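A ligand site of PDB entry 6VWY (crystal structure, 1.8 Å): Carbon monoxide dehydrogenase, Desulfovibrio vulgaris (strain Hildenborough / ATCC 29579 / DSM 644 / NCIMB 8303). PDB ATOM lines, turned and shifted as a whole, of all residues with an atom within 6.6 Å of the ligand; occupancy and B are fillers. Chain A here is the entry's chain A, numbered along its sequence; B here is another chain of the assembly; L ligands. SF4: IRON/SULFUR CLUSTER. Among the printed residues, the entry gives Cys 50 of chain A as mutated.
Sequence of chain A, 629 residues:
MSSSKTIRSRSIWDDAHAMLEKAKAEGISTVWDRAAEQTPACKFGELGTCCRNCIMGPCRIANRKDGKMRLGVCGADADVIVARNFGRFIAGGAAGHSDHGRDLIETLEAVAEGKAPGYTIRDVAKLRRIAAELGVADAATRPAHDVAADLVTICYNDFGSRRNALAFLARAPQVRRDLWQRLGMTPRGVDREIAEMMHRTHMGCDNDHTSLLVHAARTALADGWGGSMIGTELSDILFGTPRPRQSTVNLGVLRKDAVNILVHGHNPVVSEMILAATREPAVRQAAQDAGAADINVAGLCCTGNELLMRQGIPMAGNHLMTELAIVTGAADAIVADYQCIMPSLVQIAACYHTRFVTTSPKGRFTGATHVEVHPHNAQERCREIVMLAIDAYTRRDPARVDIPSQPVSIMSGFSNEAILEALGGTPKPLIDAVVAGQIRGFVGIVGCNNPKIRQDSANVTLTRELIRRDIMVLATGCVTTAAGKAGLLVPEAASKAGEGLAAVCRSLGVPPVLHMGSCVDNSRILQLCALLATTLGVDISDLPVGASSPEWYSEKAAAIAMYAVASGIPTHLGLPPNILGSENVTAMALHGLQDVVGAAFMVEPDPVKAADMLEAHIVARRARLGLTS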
ATOM      1  N   CYS A  50      -0.375 -12.639  20.138  1.00  0.00           N
ATOM      2  CA  CYS A  50       0.376 -11.493  19.669  1.00  0.00           C
ATOM      3  C   CYS A  50       1.776 -11.987  19.371  1.00  0.00           C
ATOM      4  O   CYS A  50       2.328 -12.791  20.134  1.00  0.00           O
ATOM      5  CB  CYS A  50       0.438 -10.383  20.737  1.00  0.00           C
ATOM      6  SG  CYS A  50       1.719  -9.143  20.373  1.00  0.00           S
ATOM      7  N   CYS A  51       2.342 -11.539  18.264  1.00  0.00           N
ATOM      8  CA  CYS A  51       3.670 -11.976  17.859  1.00  0.00           C
ATOM      9  C   CYS A  51       4.503 -10.757  17.512  1.00  0.00           C
ATOM     10  O   CYS A  51       4.040  -9.861  16.793  1.00  0.00           O
ATOM     11  CB  CYS A  51       3.612 -12.949  16.666  1.00  0.00           C
ATOM     12  SG  CYS A  51       5.272 -13.661  16.291  1.00  0.00           S
ATOM     13  N   ARG A  52       5.722 -10.717  18.034  1.00  0.00           N
ATOM     14  CA  ARG A  52       6.665  -9.647  17.741  1.00  0.00           C
ATOM     15  C   ARG A  52       8.029 -10.220  17.349  1.00  0.00           C
ATOM     16  O   ARG A  52       9.052  -9.605  17.618  1.00  0.00           O
ATOM     17  CB  ARG A  52       6.823  -8.695  18.929  1.00  0.00           C
ATOM     18  CG  ARG A  52       5.509  -8.157  19.525  1.00  0.00           C
ATOM     19  CD  ARG A  52       5.788  -7.302  20.774  1.00  0.00           C
ATOM     20  NE  ARG A  52       6.010  -8.143  21.946  1.00  0.00           N
ATOM     21  CZ  ARG A  52       6.618  -7.728  23.053  1.00  0.00           C
ATOM     22  NH1 ARG A  52       7.094  -6.482  23.125  1.00  0.00           N
ATOM     23  NH2 ARG A  52       6.771  -8.566  24.082  1.00  0.00           N
ATOM     24  N   ASN A  53       8.042 -11.395  16.726  1.00  0.00           N
ATOM     25  CA  ASN A  53       9.303 -12.091  16.444  1.00  0.00           C
ATOM     26  C   ASN A  53      10.014 -11.587  15.187  1.00  0.00           C
ATOM     27  O   ASN A  53      11.098 -12.082  14.892  1.00  0.00           O
ATOM     28  CB  ASN A  53       9.062 -13.591  16.333  1.00  0.00           C
ATOM     29  CG  ASN A  53       8.731 -14.230  17.676  1.00  0.00           C
ATOM     30  OD1 ASN A  53       8.522 -13.536  18.655  1.00  0.00           O
ATOM     31  ND2 ASN A  53       8.684 -15.565  17.713  1.00  0.00           N
ATOM     32  N   CYS A  54       9.431 -10.638  14.452  1.00  0.00           N
ATOM     33  CA  CYS A  54      10.143  -9.982  13.360  1.00  0.00           C
ATOM     34  C   CYS A  54       9.492  -8.620  13.155  1.00  0.00           C
ATOM     35  O   CYS A  54       8.450  -8.344  13.729  1.00  0.00           O
ATOM     36  CB  CYS A  54      10.120 -10.837  12.083  1.00  0.00           C
ATOM     37  SG  CYS A  54       8.572 -10.777  11.123  1.00  0.00           S
ATOM     38  N   ILE A  55      10.114  -7.768  12.331  1.00  0.00           N
ATOM     39  CA  ILE A  55       9.551  -6.434  12.122  1.00  0.00           C
ATOM     40  C   ILE A  55       8.746  -6.357  10.819  1.00  0.00           C
ATOM     41  O   ILE A  55       8.463  -5.257  10.339  1.00  0.00           O
ATOM     42  CB  ILE A  55      10.602  -5.308  12.200  1.00  0.00           C
ATOM     43  CG1 ILE A  55      11.632  -5.381  11.082  1.00  0.00           C
ATOM     44  CG2 ILE A  55      11.283  -5.284  13.577  1.00  0.00           C
ATOM     45  CD1 ILE A  55      12.170  -3.999  10.690  1.00  0.00           C
ATOM     46  N   MET A  56       8.331  -7.496  10.249  1.00  0.00           N
ATOM     47  CA  MET A  56       7.077  -7.460   9.492  1.00  0.00           C
ATOM     48  C   MET A  56       5.902  -7.290  10.441  1.00  0.00           C
ATOM     49  O   MET A  56       4.862  -6.742  10.065  1.00  0.00           O
ATOM     50  CB  MET A  56       6.894  -8.732   8.648  1.00  0.00           C
ATOM     51  CG  MET A  56       7.971  -8.915   7.579  1.00  0.00           C
ATOM     52  SD  MET A  56       7.464 -10.056   6.257  1.00  0.00           S
ATOM     53  CE  MET A  56       7.291 -11.615   7.124  1.00  0.00           C
ATOM     54  N   GLY A  57       6.071  -7.719  11.685  1.00  0.00           N
ATOM     55  CA  GLY A  57       5.119  -7.428  12.734  1.00  0.00           C
ATOM     56  C   GLY A  57       5.331  -6.049  13.328  1.00  0.00           C
ATOM     57  O   GLY A  57       6.051  -5.209  12.769  1.00  0.00           O
ATOM     58  N   PRO A  58       4.708  -5.784  14.490  1.00  0.00           N
ATOM     59  CA  PRO A  58       3.939  -6.721  15.314  1.00  0.00           C
ATOM     60  C   PRO A  58       2.668  -7.258  14.653  1.00  0.00           C
ATOM     61  O   PRO A  58       2.028  -6.559  13.882  1.00  0.00           O
ATOM     62  CB  PRO A  58       3.576  -5.889  16.552  1.00  0.00           C
ATOM     63  CG  PRO A  58       4.529  -4.741  16.561  1.00  0.00           C
ATOM     64  CD  PRO A  58       4.790  -4.443  15.114  1.00  0.00           C
ATOM     65  N   CYS A  59       2.303  -8.490  14.996  1.00  0.00           N
ATOM     66  CA  CYS A  59       1.088  -9.108  14.500  1.00  0.00           C
ATOM     67  C   CYS A  59       0.206  -9.488  15.661  1.00  0.00           C
ATOM     68  O   CYS A  59       0.689  -9.862  16.740  1.00  0.00           O
ATOM     69  CB  CYS A  59       1.404 -10.346  13.662  1.00  0.00           C
ATOM     70  SG  CYS A  59       2.437  -9.984  12.205  1.00  0.00           S
ATOM     71  N   ARG A  60      -1.106  -9.393  15.457  1.00  0.00           N
ATOM     72  CA  ARG A  60      -2.031  -9.939  16.434  1.00  0.00           C
ATOM     73  C   ARG A  60      -3.141 -10.674  15.699  1.00  0.00           C
ATOM     74  O   ARG A  60      -3.534 -10.291  14.595  1.00  0.00           O
ATOM     75  CB  ARG A  60      -2.596  -8.841  17.352  1.00  0.00           C
ATOM     76  CG  ARG A  60      -3.302  -7.706  16.644  1.00  0.00           C
ATOM     77  CD  ARG A  60      -3.573  -6.508  17.582  1.00  0.00           C
ATOM     78  NE  ARG A  60      -4.619  -5.664  17.012  1.00  0.00           N
ATOM     79  CZ  ARG A  60      -4.407  -4.709  16.109  1.00  0.00           C
ATOM     80  NH1 ARG A  60      -5.436  -4.016  15.638  1.00  0.00           N
ATOM     81  NH2 ARG A  60      -3.178  -4.456  15.667  1.00  0.00           N
ATOM     82  N   ILE A  61      -3.619 -11.757  16.312  1.00  0.00           N
ATOM     83  CA  ILE A  61      -4.596 -12.657  15.713  1.00  0.00           C
ATOM     84  C   ILE A  61      -5.920 -12.427  16.400  1.00  0.00           C
ATOM     85  O   ILE A  61      -6.031 -12.570  17.626  1.00  0.00           O
ATOM     86  CB  ILE A  61      -4.171 -14.134  15.837  1.00  0.00           C
ATOM     87  CG1 ILE A  61      -2.741 -14.328  15.327  1.00  0.00           C
ATOM     88  CG2 ILE A  61      -5.171 -15.038  15.121  1.00  0.00           C
ATOM     89  CD1 ILE A  61      -2.557 -13.938  13.856  1.00  0.00           C
ATOM     90  N   LEU A  71      -4.186 -14.456  10.295  1.00  0.00           N
ATOM     91  CA  LEU A  71      -2.804 -14.869  10.160  1.00  0.00           C
ATOM     92  C   LEU A  71      -1.879 -13.685  10.387  1.00  0.00           C
ATOM     93  O   LEU A  71      -2.244 -12.538  10.147  1.00  0.00           O
ATOM     94  CB  LEU A  71      -2.541 -15.466   8.760  1.00  0.00           C
ATOM     95  CG  LEU A  71      -3.473 -16.595   8.285  1.00  0.00           C
ATOM     96  CD1 LEU A  71      -3.217 -16.953   6.803  1.00  0.00           C
ATOM     97  CD2 LEU A  71      -3.312 -17.814   9.187  1.00  0.00           C
ATOM     98  N   GLY A  72      -0.670 -13.971  10.848  1.00  0.00           N
ATOM     99  CA  GLY A  72       0.360 -12.942  10.900  1.00  0.00           C
ATOM    100  C   GLY A  72       0.825 -12.599   9.491  1.00  0.00           C
ATOM    101  O   GLY A  72       0.422 -13.197   8.499  1.00  0.00           O
ATOM    102  N   VAL A  73       1.712 -11.608   9.405  1.00  0.00           N
ATOM    103  CA  VAL A  73       2.128 -11.166   8.066  1.00  0.00           C
ATOM    104  C   VAL A  73       2.822 -12.301   7.316  1.00  0.00           C
ATOM    105  O   VAL A  73       2.642 -12.466   6.102  1.00  0.00           O
ATOM    106  CB  VAL A  73       3.001  -9.906   8.160  1.00  0.00           C
ATOM    107  CG1 VAL A  73       3.520  -9.511   6.761  1.00  0.00           C
ATOM    108  CG2 VAL A  73       2.212  -8.747   8.768  1.00  0.00           C
ATOM    109  N   CYS A  74       3.583 -13.137   8.035  1.00  0.00           N
ATOM    110  CA  CYS A  74       4.243 -14.285   7.402  1.00  0.00           C
ATOM    111  C   CYS A  74       3.280 -15.424   7.095  1.00  0.00           C
ATOM    112  O   CYS A  74       3.699 -16.421   6.510  1.00  0.00           O
ATOM    113  CB  CYS A  74       5.367 -14.817   8.295  1.00  0.00           C
ATOM    114  SG  CYS A  74       4.738 -15.496   9.915  1.00  0.00           S
ATOM    115  N   GLY A  75       2.025 -15.337   7.527  1.00  0.00           N
ATOM    116  CA  GLY A  75       1.080 -16.432   7.366  1.00  0.00           C
ATOM    117  C   GLY A  75       0.877 -17.303   8.591  1.00  0.00           C
ATOM    118  O   GLY A  75       0.079 -18.257   8.517  1.00  0.00           O
ATOM    119  N   ALA A  76       1.572 -17.046   9.690  1.00  0.00           N
ATOM    120  CA  ALA A  76       1.434 -17.894  10.873  1.00  0.00           C
ATOM    121  C   ALA A  76       0.065 -17.705  11.515  1.00  0.00           C
ATOM    122  O   ALA A  76      -0.432 -16.580  11.647  1.00  0.00           O
ATOM    123  CB  ALA A  76       2.548 -17.570  11.887  1.00  0.00           C
ATOM    124  N   ILE A  81       1.530 -19.180  16.587  1.00  0.00           N
ATOM    125  CA  ILE A  81       1.974 -18.009  17.348  1.00  0.00           C
ATOM    126  C   ILE A  81       1.925 -18.303  18.846  1.00  0.00           C
ATOM    127  O   ILE A  81       2.895 -18.033  19.579  1.00  0.00           O
ATOM    128  CB  ILE A  81       1.128 -16.784  16.977  1.00  0.00           C
ATOM    129  CG1 ILE A  81       1.594 -16.248  15.605  1.00  0.00           C
ATOM    130  CG2 ILE A  81       1.242 -15.709  18.051  1.00  0.00           C
ATOM    131  CD1 ILE A  81       0.592 -15.352  14.919  1.00  0.00           C
ATOM    132  N   ARG A  84       4.679 -20.935  19.710  1.00  0.00           N
ATOM    133  CA  ARG A  84       6.020 -20.340  19.743  1.00  0.00           C
ATOM    134  C   ARG A  84       6.203 -19.459  20.976  1.00  0.00           C
ATOM    135  O   ARG A  84       7.269 -19.493  21.610  1.00  0.00           O
ATOM    136  CB  ARG A  84       6.290 -19.521  18.477  1.00  0.00           C
ATOM    137  CG  ARG A  84       6.380 -20.376  17.211  1.00  0.00           C
ATOM    138  CD  ARG A  84       6.917 -19.578  16.008  1.00  0.00           C
ATOM    139  NE  ARG A  84       6.119 -18.384  15.734  1.00  0.00           N
ATOM    140  CZ  ARG A  84       6.025 -17.792  14.543  1.00  0.00           C
ATOM    141  NH1 ARG A  84       6.664 -18.319  13.503  1.00  0.00           N
ATOM    142  NH2 ARG A  84       5.277 -16.705  14.369  1.00  0.00           N
ATOM    143  N   THR A 201      11.632 -20.913  16.964  1.00  0.00           N
ATOM    144  CA  THR A 201      10.600 -19.890  17.076  1.00  0.00           C
ATOM    145  C   THR A 201      10.885 -18.650  16.231  1.00  0.00           C
ATOM    146  O   THR A 201      10.043 -17.738  16.225  1.00  0.00           O
ATOM    147  CB  THR A 201      10.399 -19.529  18.552  1.00  0.00           C
ATOM    148  OG1 THR A 201      11.679 -19.238  19.152  1.00  0.00           O
ATOM    149  CG2 THR A 201       9.779 -20.718  19.288  1.00  0.00           C
ATOM    150  N   HIS A 202      12.013 -18.599  15.525  1.00  0.00           N
ATOM    151  CA  HIS A 202      12.260 -17.592  14.494  1.00  0.00           C
ATOM    152  C   HIS A 202      11.211 -17.720  13.397  1.00  0.00           C
ATOM    153  O   HIS A 202      10.703 -18.814  13.130  1.00  0.00           O
ATOM    154  CB  HIS A 202      13.670 -17.789  13.910  1.00  0.00           C
ATOM    155  CG  HIS A 202      14.142 -16.676  13.005  1.00  0.00           C
ATOM    156  ND1 HIS A 202      13.648 -16.469  11.734  1.00  0.00           N
ATOM    157  CD2 HIS A 202      15.088 -15.726  13.189  1.00  0.00           C
ATOM    158  CE1 HIS A 202      14.261 -15.433  11.180  1.00  0.00           C
ATOM    159  NE2 HIS A 202      15.145 -14.961  12.045  1.00  0.00           N
ATOM    160  N   MET A 203      10.900 -16.610  12.723  1.00  0.00           N
ATOM    161  CA  MET A 203       9.959 -16.659  11.601  1.00  0.00           C
ATOM    162  C   MET A 203      10.368 -17.745  10.632  1.00  0.00           C
ATOM    163  O   MET A 203      11.556 -17.901  10.309  1.00  0.00           O
ATOM    164  CB  MET A 203       9.876 -15.325  10.850  1.00  0.00           C
ATOM    165  CG  MET A 203       8.761 -15.222   9.814  1.00  0.00           C
ATOM    166  SD  MET A 203       8.975 -16.164   8.239  1.00  0.00           S
ATOM    167  CE  MET A 203       9.246 -14.819   7.089  1.00  0.00           C
ATOM    168  N   GLY A 204       9.382 -18.509  10.170  1.00  0.00           N
ATOM    169  CA  GLY A 204       9.625 -19.428   9.073  1.00  0.00           C
ATOM    170  C   GLY A 204      10.511 -20.596   9.420  1.00  0.00           C
ATOM    171  O   GLY A 204      11.182 -21.133   8.543  1.00  0.00           O
ATOM    172  N   GLN B  38      -2.654  -6.097   9.081  1.00  0.00           N
ATOM    173  CA  GLN B  38      -2.002  -5.883  10.368  1.00  0.00           C
ATOM    174  C   GLN B  38      -1.568  -4.428  10.572  1.00  0.00           C
ATOM    175  O   GLN B  38      -0.758  -4.142  11.464  1.00  0.00           O
ATOM    176  CB  GLN B  38      -0.806  -6.833  10.512  1.00  0.00           C
ATOM    177  CG  GLN B  38      -1.194  -8.331  10.523  1.00  0.00           C
ATOM    178  CD  GLN B  38      -1.822  -8.755  11.847  1.00  0.00           C
ATOM    179  OE1 GLN B  38      -1.674  -8.074  12.863  1.00  0.00           O
ATOM    180  NE2 GLN B  38      -2.510  -9.888  11.837  1.00  0.00           N
ATOM    181  N   PRO B 343       4.917 -19.594   6.238  1.00  0.00           N
ATOM    182  CA  PRO B 343       3.935 -20.690   6.231  1.00  0.00           C
ATOM    183  C   PRO B 343       2.782 -20.479   5.274  1.00  0.00           C
ATOM    184  O   PRO B 343       2.109 -21.461   4.917  1.00  0.00           O
ATOM    185  CB  PRO B 343       3.466 -20.768   7.698  1.00  0.00           C
ATOM    186  CG  PRO B 343       3.874 -19.437   8.293  1.00  0.00           C
ATOM    187  CD  PRO B 343       5.094 -18.996   7.575  1.00  0.00           C
ATOM    188  N   TYR B 553      13.985  -7.477   7.874  1.00  0.00           N
ATOM    189  CA  TYR B 553      12.811  -7.861   8.653  1.00  0.00           C
ATOM    190  C   TYR B 553      13.120  -8.818   9.815  1.00  0.00           C
ATOM    191  O   TYR B 553      12.418  -8.750  10.839  1.00  0.00           O
ATOM    192  CB  TYR B 553      11.726  -8.504   7.726  1.00  0.00           C
ATOM    193  CG  TYR B 553      11.817 -10.021   7.725  1.00  0.00           C
ATOM    194  CD1 TYR B 553      11.184 -10.755   8.733  1.00  0.00           C
ATOM    195  CD2 TYR B 553      12.557 -10.710   6.764  1.00  0.00           C
ATOM    196  CE1 TYR B 553      11.285 -12.107   8.799  1.00  0.00           C
ATOM    197  CE2 TYR B 553      12.649 -12.103   6.821  1.00  0.00           C
ATOM    198  CZ  TYR B 553      12.014 -12.787   7.855  1.00  0.00           C
ATOM    199  OH  TYR B 553      12.102 -14.149   7.986  1.00  0.00           O
HETATM  200 FE1  SF4 L   1       5.447 -13.096  14.096  1.00  0.00          FE
HETATM  201 FE2  SF4 L   1       4.136 -11.457  12.416  1.00  0.00          FE
HETATM  202 FE3  SF4 L   1       5.168 -13.874  11.494  1.00  0.00          FE
HETATM  203 FE4  SF4 L   1       6.848 -11.817  12.171  1.00  0.00          FE
HETATM  204  S1  SF4 L   1       5.295 -11.808  10.493  1.00  0.00           S
HETATM  205  S2  SF4 L   1       7.066 -13.986  12.775  1.00  0.00           S
HETATM  206  S3  SF4 L   1       5.751 -10.849  13.927  1.00  0.00           S
HETATM  207  S4  SF4 L   1       3.463 -13.578  13.037  1.00  0.00           S
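An iron atom (FE2) of the ligand is bound by the side-chain sulfur (SG) of Cys 59 (2.3 Å). The backbone NH of Cys 54 lies close to a sulfur (S3) of the ligand, at 3.7 Å. FE4 of the ligand is bound by SG of Cys 54 (2.3 Å). The side-chain sulfur (SG) of Cys 51 binds an iron atom (FE1) of the ligand. The backbone NH (N) of Cys 74 sits close to a sulfur (S1) of the ligand, at 3.3 Å. SG of Cys 74 binds FE3 of the ligand, 2.3 Å away. NH2 of Arg 84 sits close to S2 of the ligand (3.6 Å). N of Asn 53 lies close to S3 of the ligand (3.7 Å). The backbone NH of Val 73 sits close to a sulfur (S1) of the ligand (3.7 Å).
The backbone carbonyl oxygen of Cys 59 lies within hydrogen-bond range of the backbone NH of Cys 51 (2.8 Å). The side-chain sulfur (SG) of Cys 59 lies close to the backbone NH (N) of Val 73 (3.3 Å). SG of Cys 54 sits close to N of Met 56. SG of Cys 51 sits close to NH2 of Arg 84 (3.6 Å). The side-chain sulfur (SG) of Cys 51 sits close to the backbone NH (N) of Asn 53 (3.6 Å). The side-chain sulfur of Cys 74 lies close to the backbone NH of Ala 76 (3.5 Å). The side-chain sulfur (SD) of Met 203 sits close to the side-chain hydroxyl (OH) of Tyr 553 of chain B (3.7 Å). O of Thr 201 is in hydrogen-bond range of ND2 of Asn 53 (3.0 Å).
Residues that only touch the ligand: Met 203 (3.6 Å), Gly 57 (3.7 Å), Gly 72 (3.8 Å), Ile 81 (3.9 Å) and Met 56 (3.9 Å). The nearest printed residue that does not touch the ligand is Arg 52 (4.1 Å).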
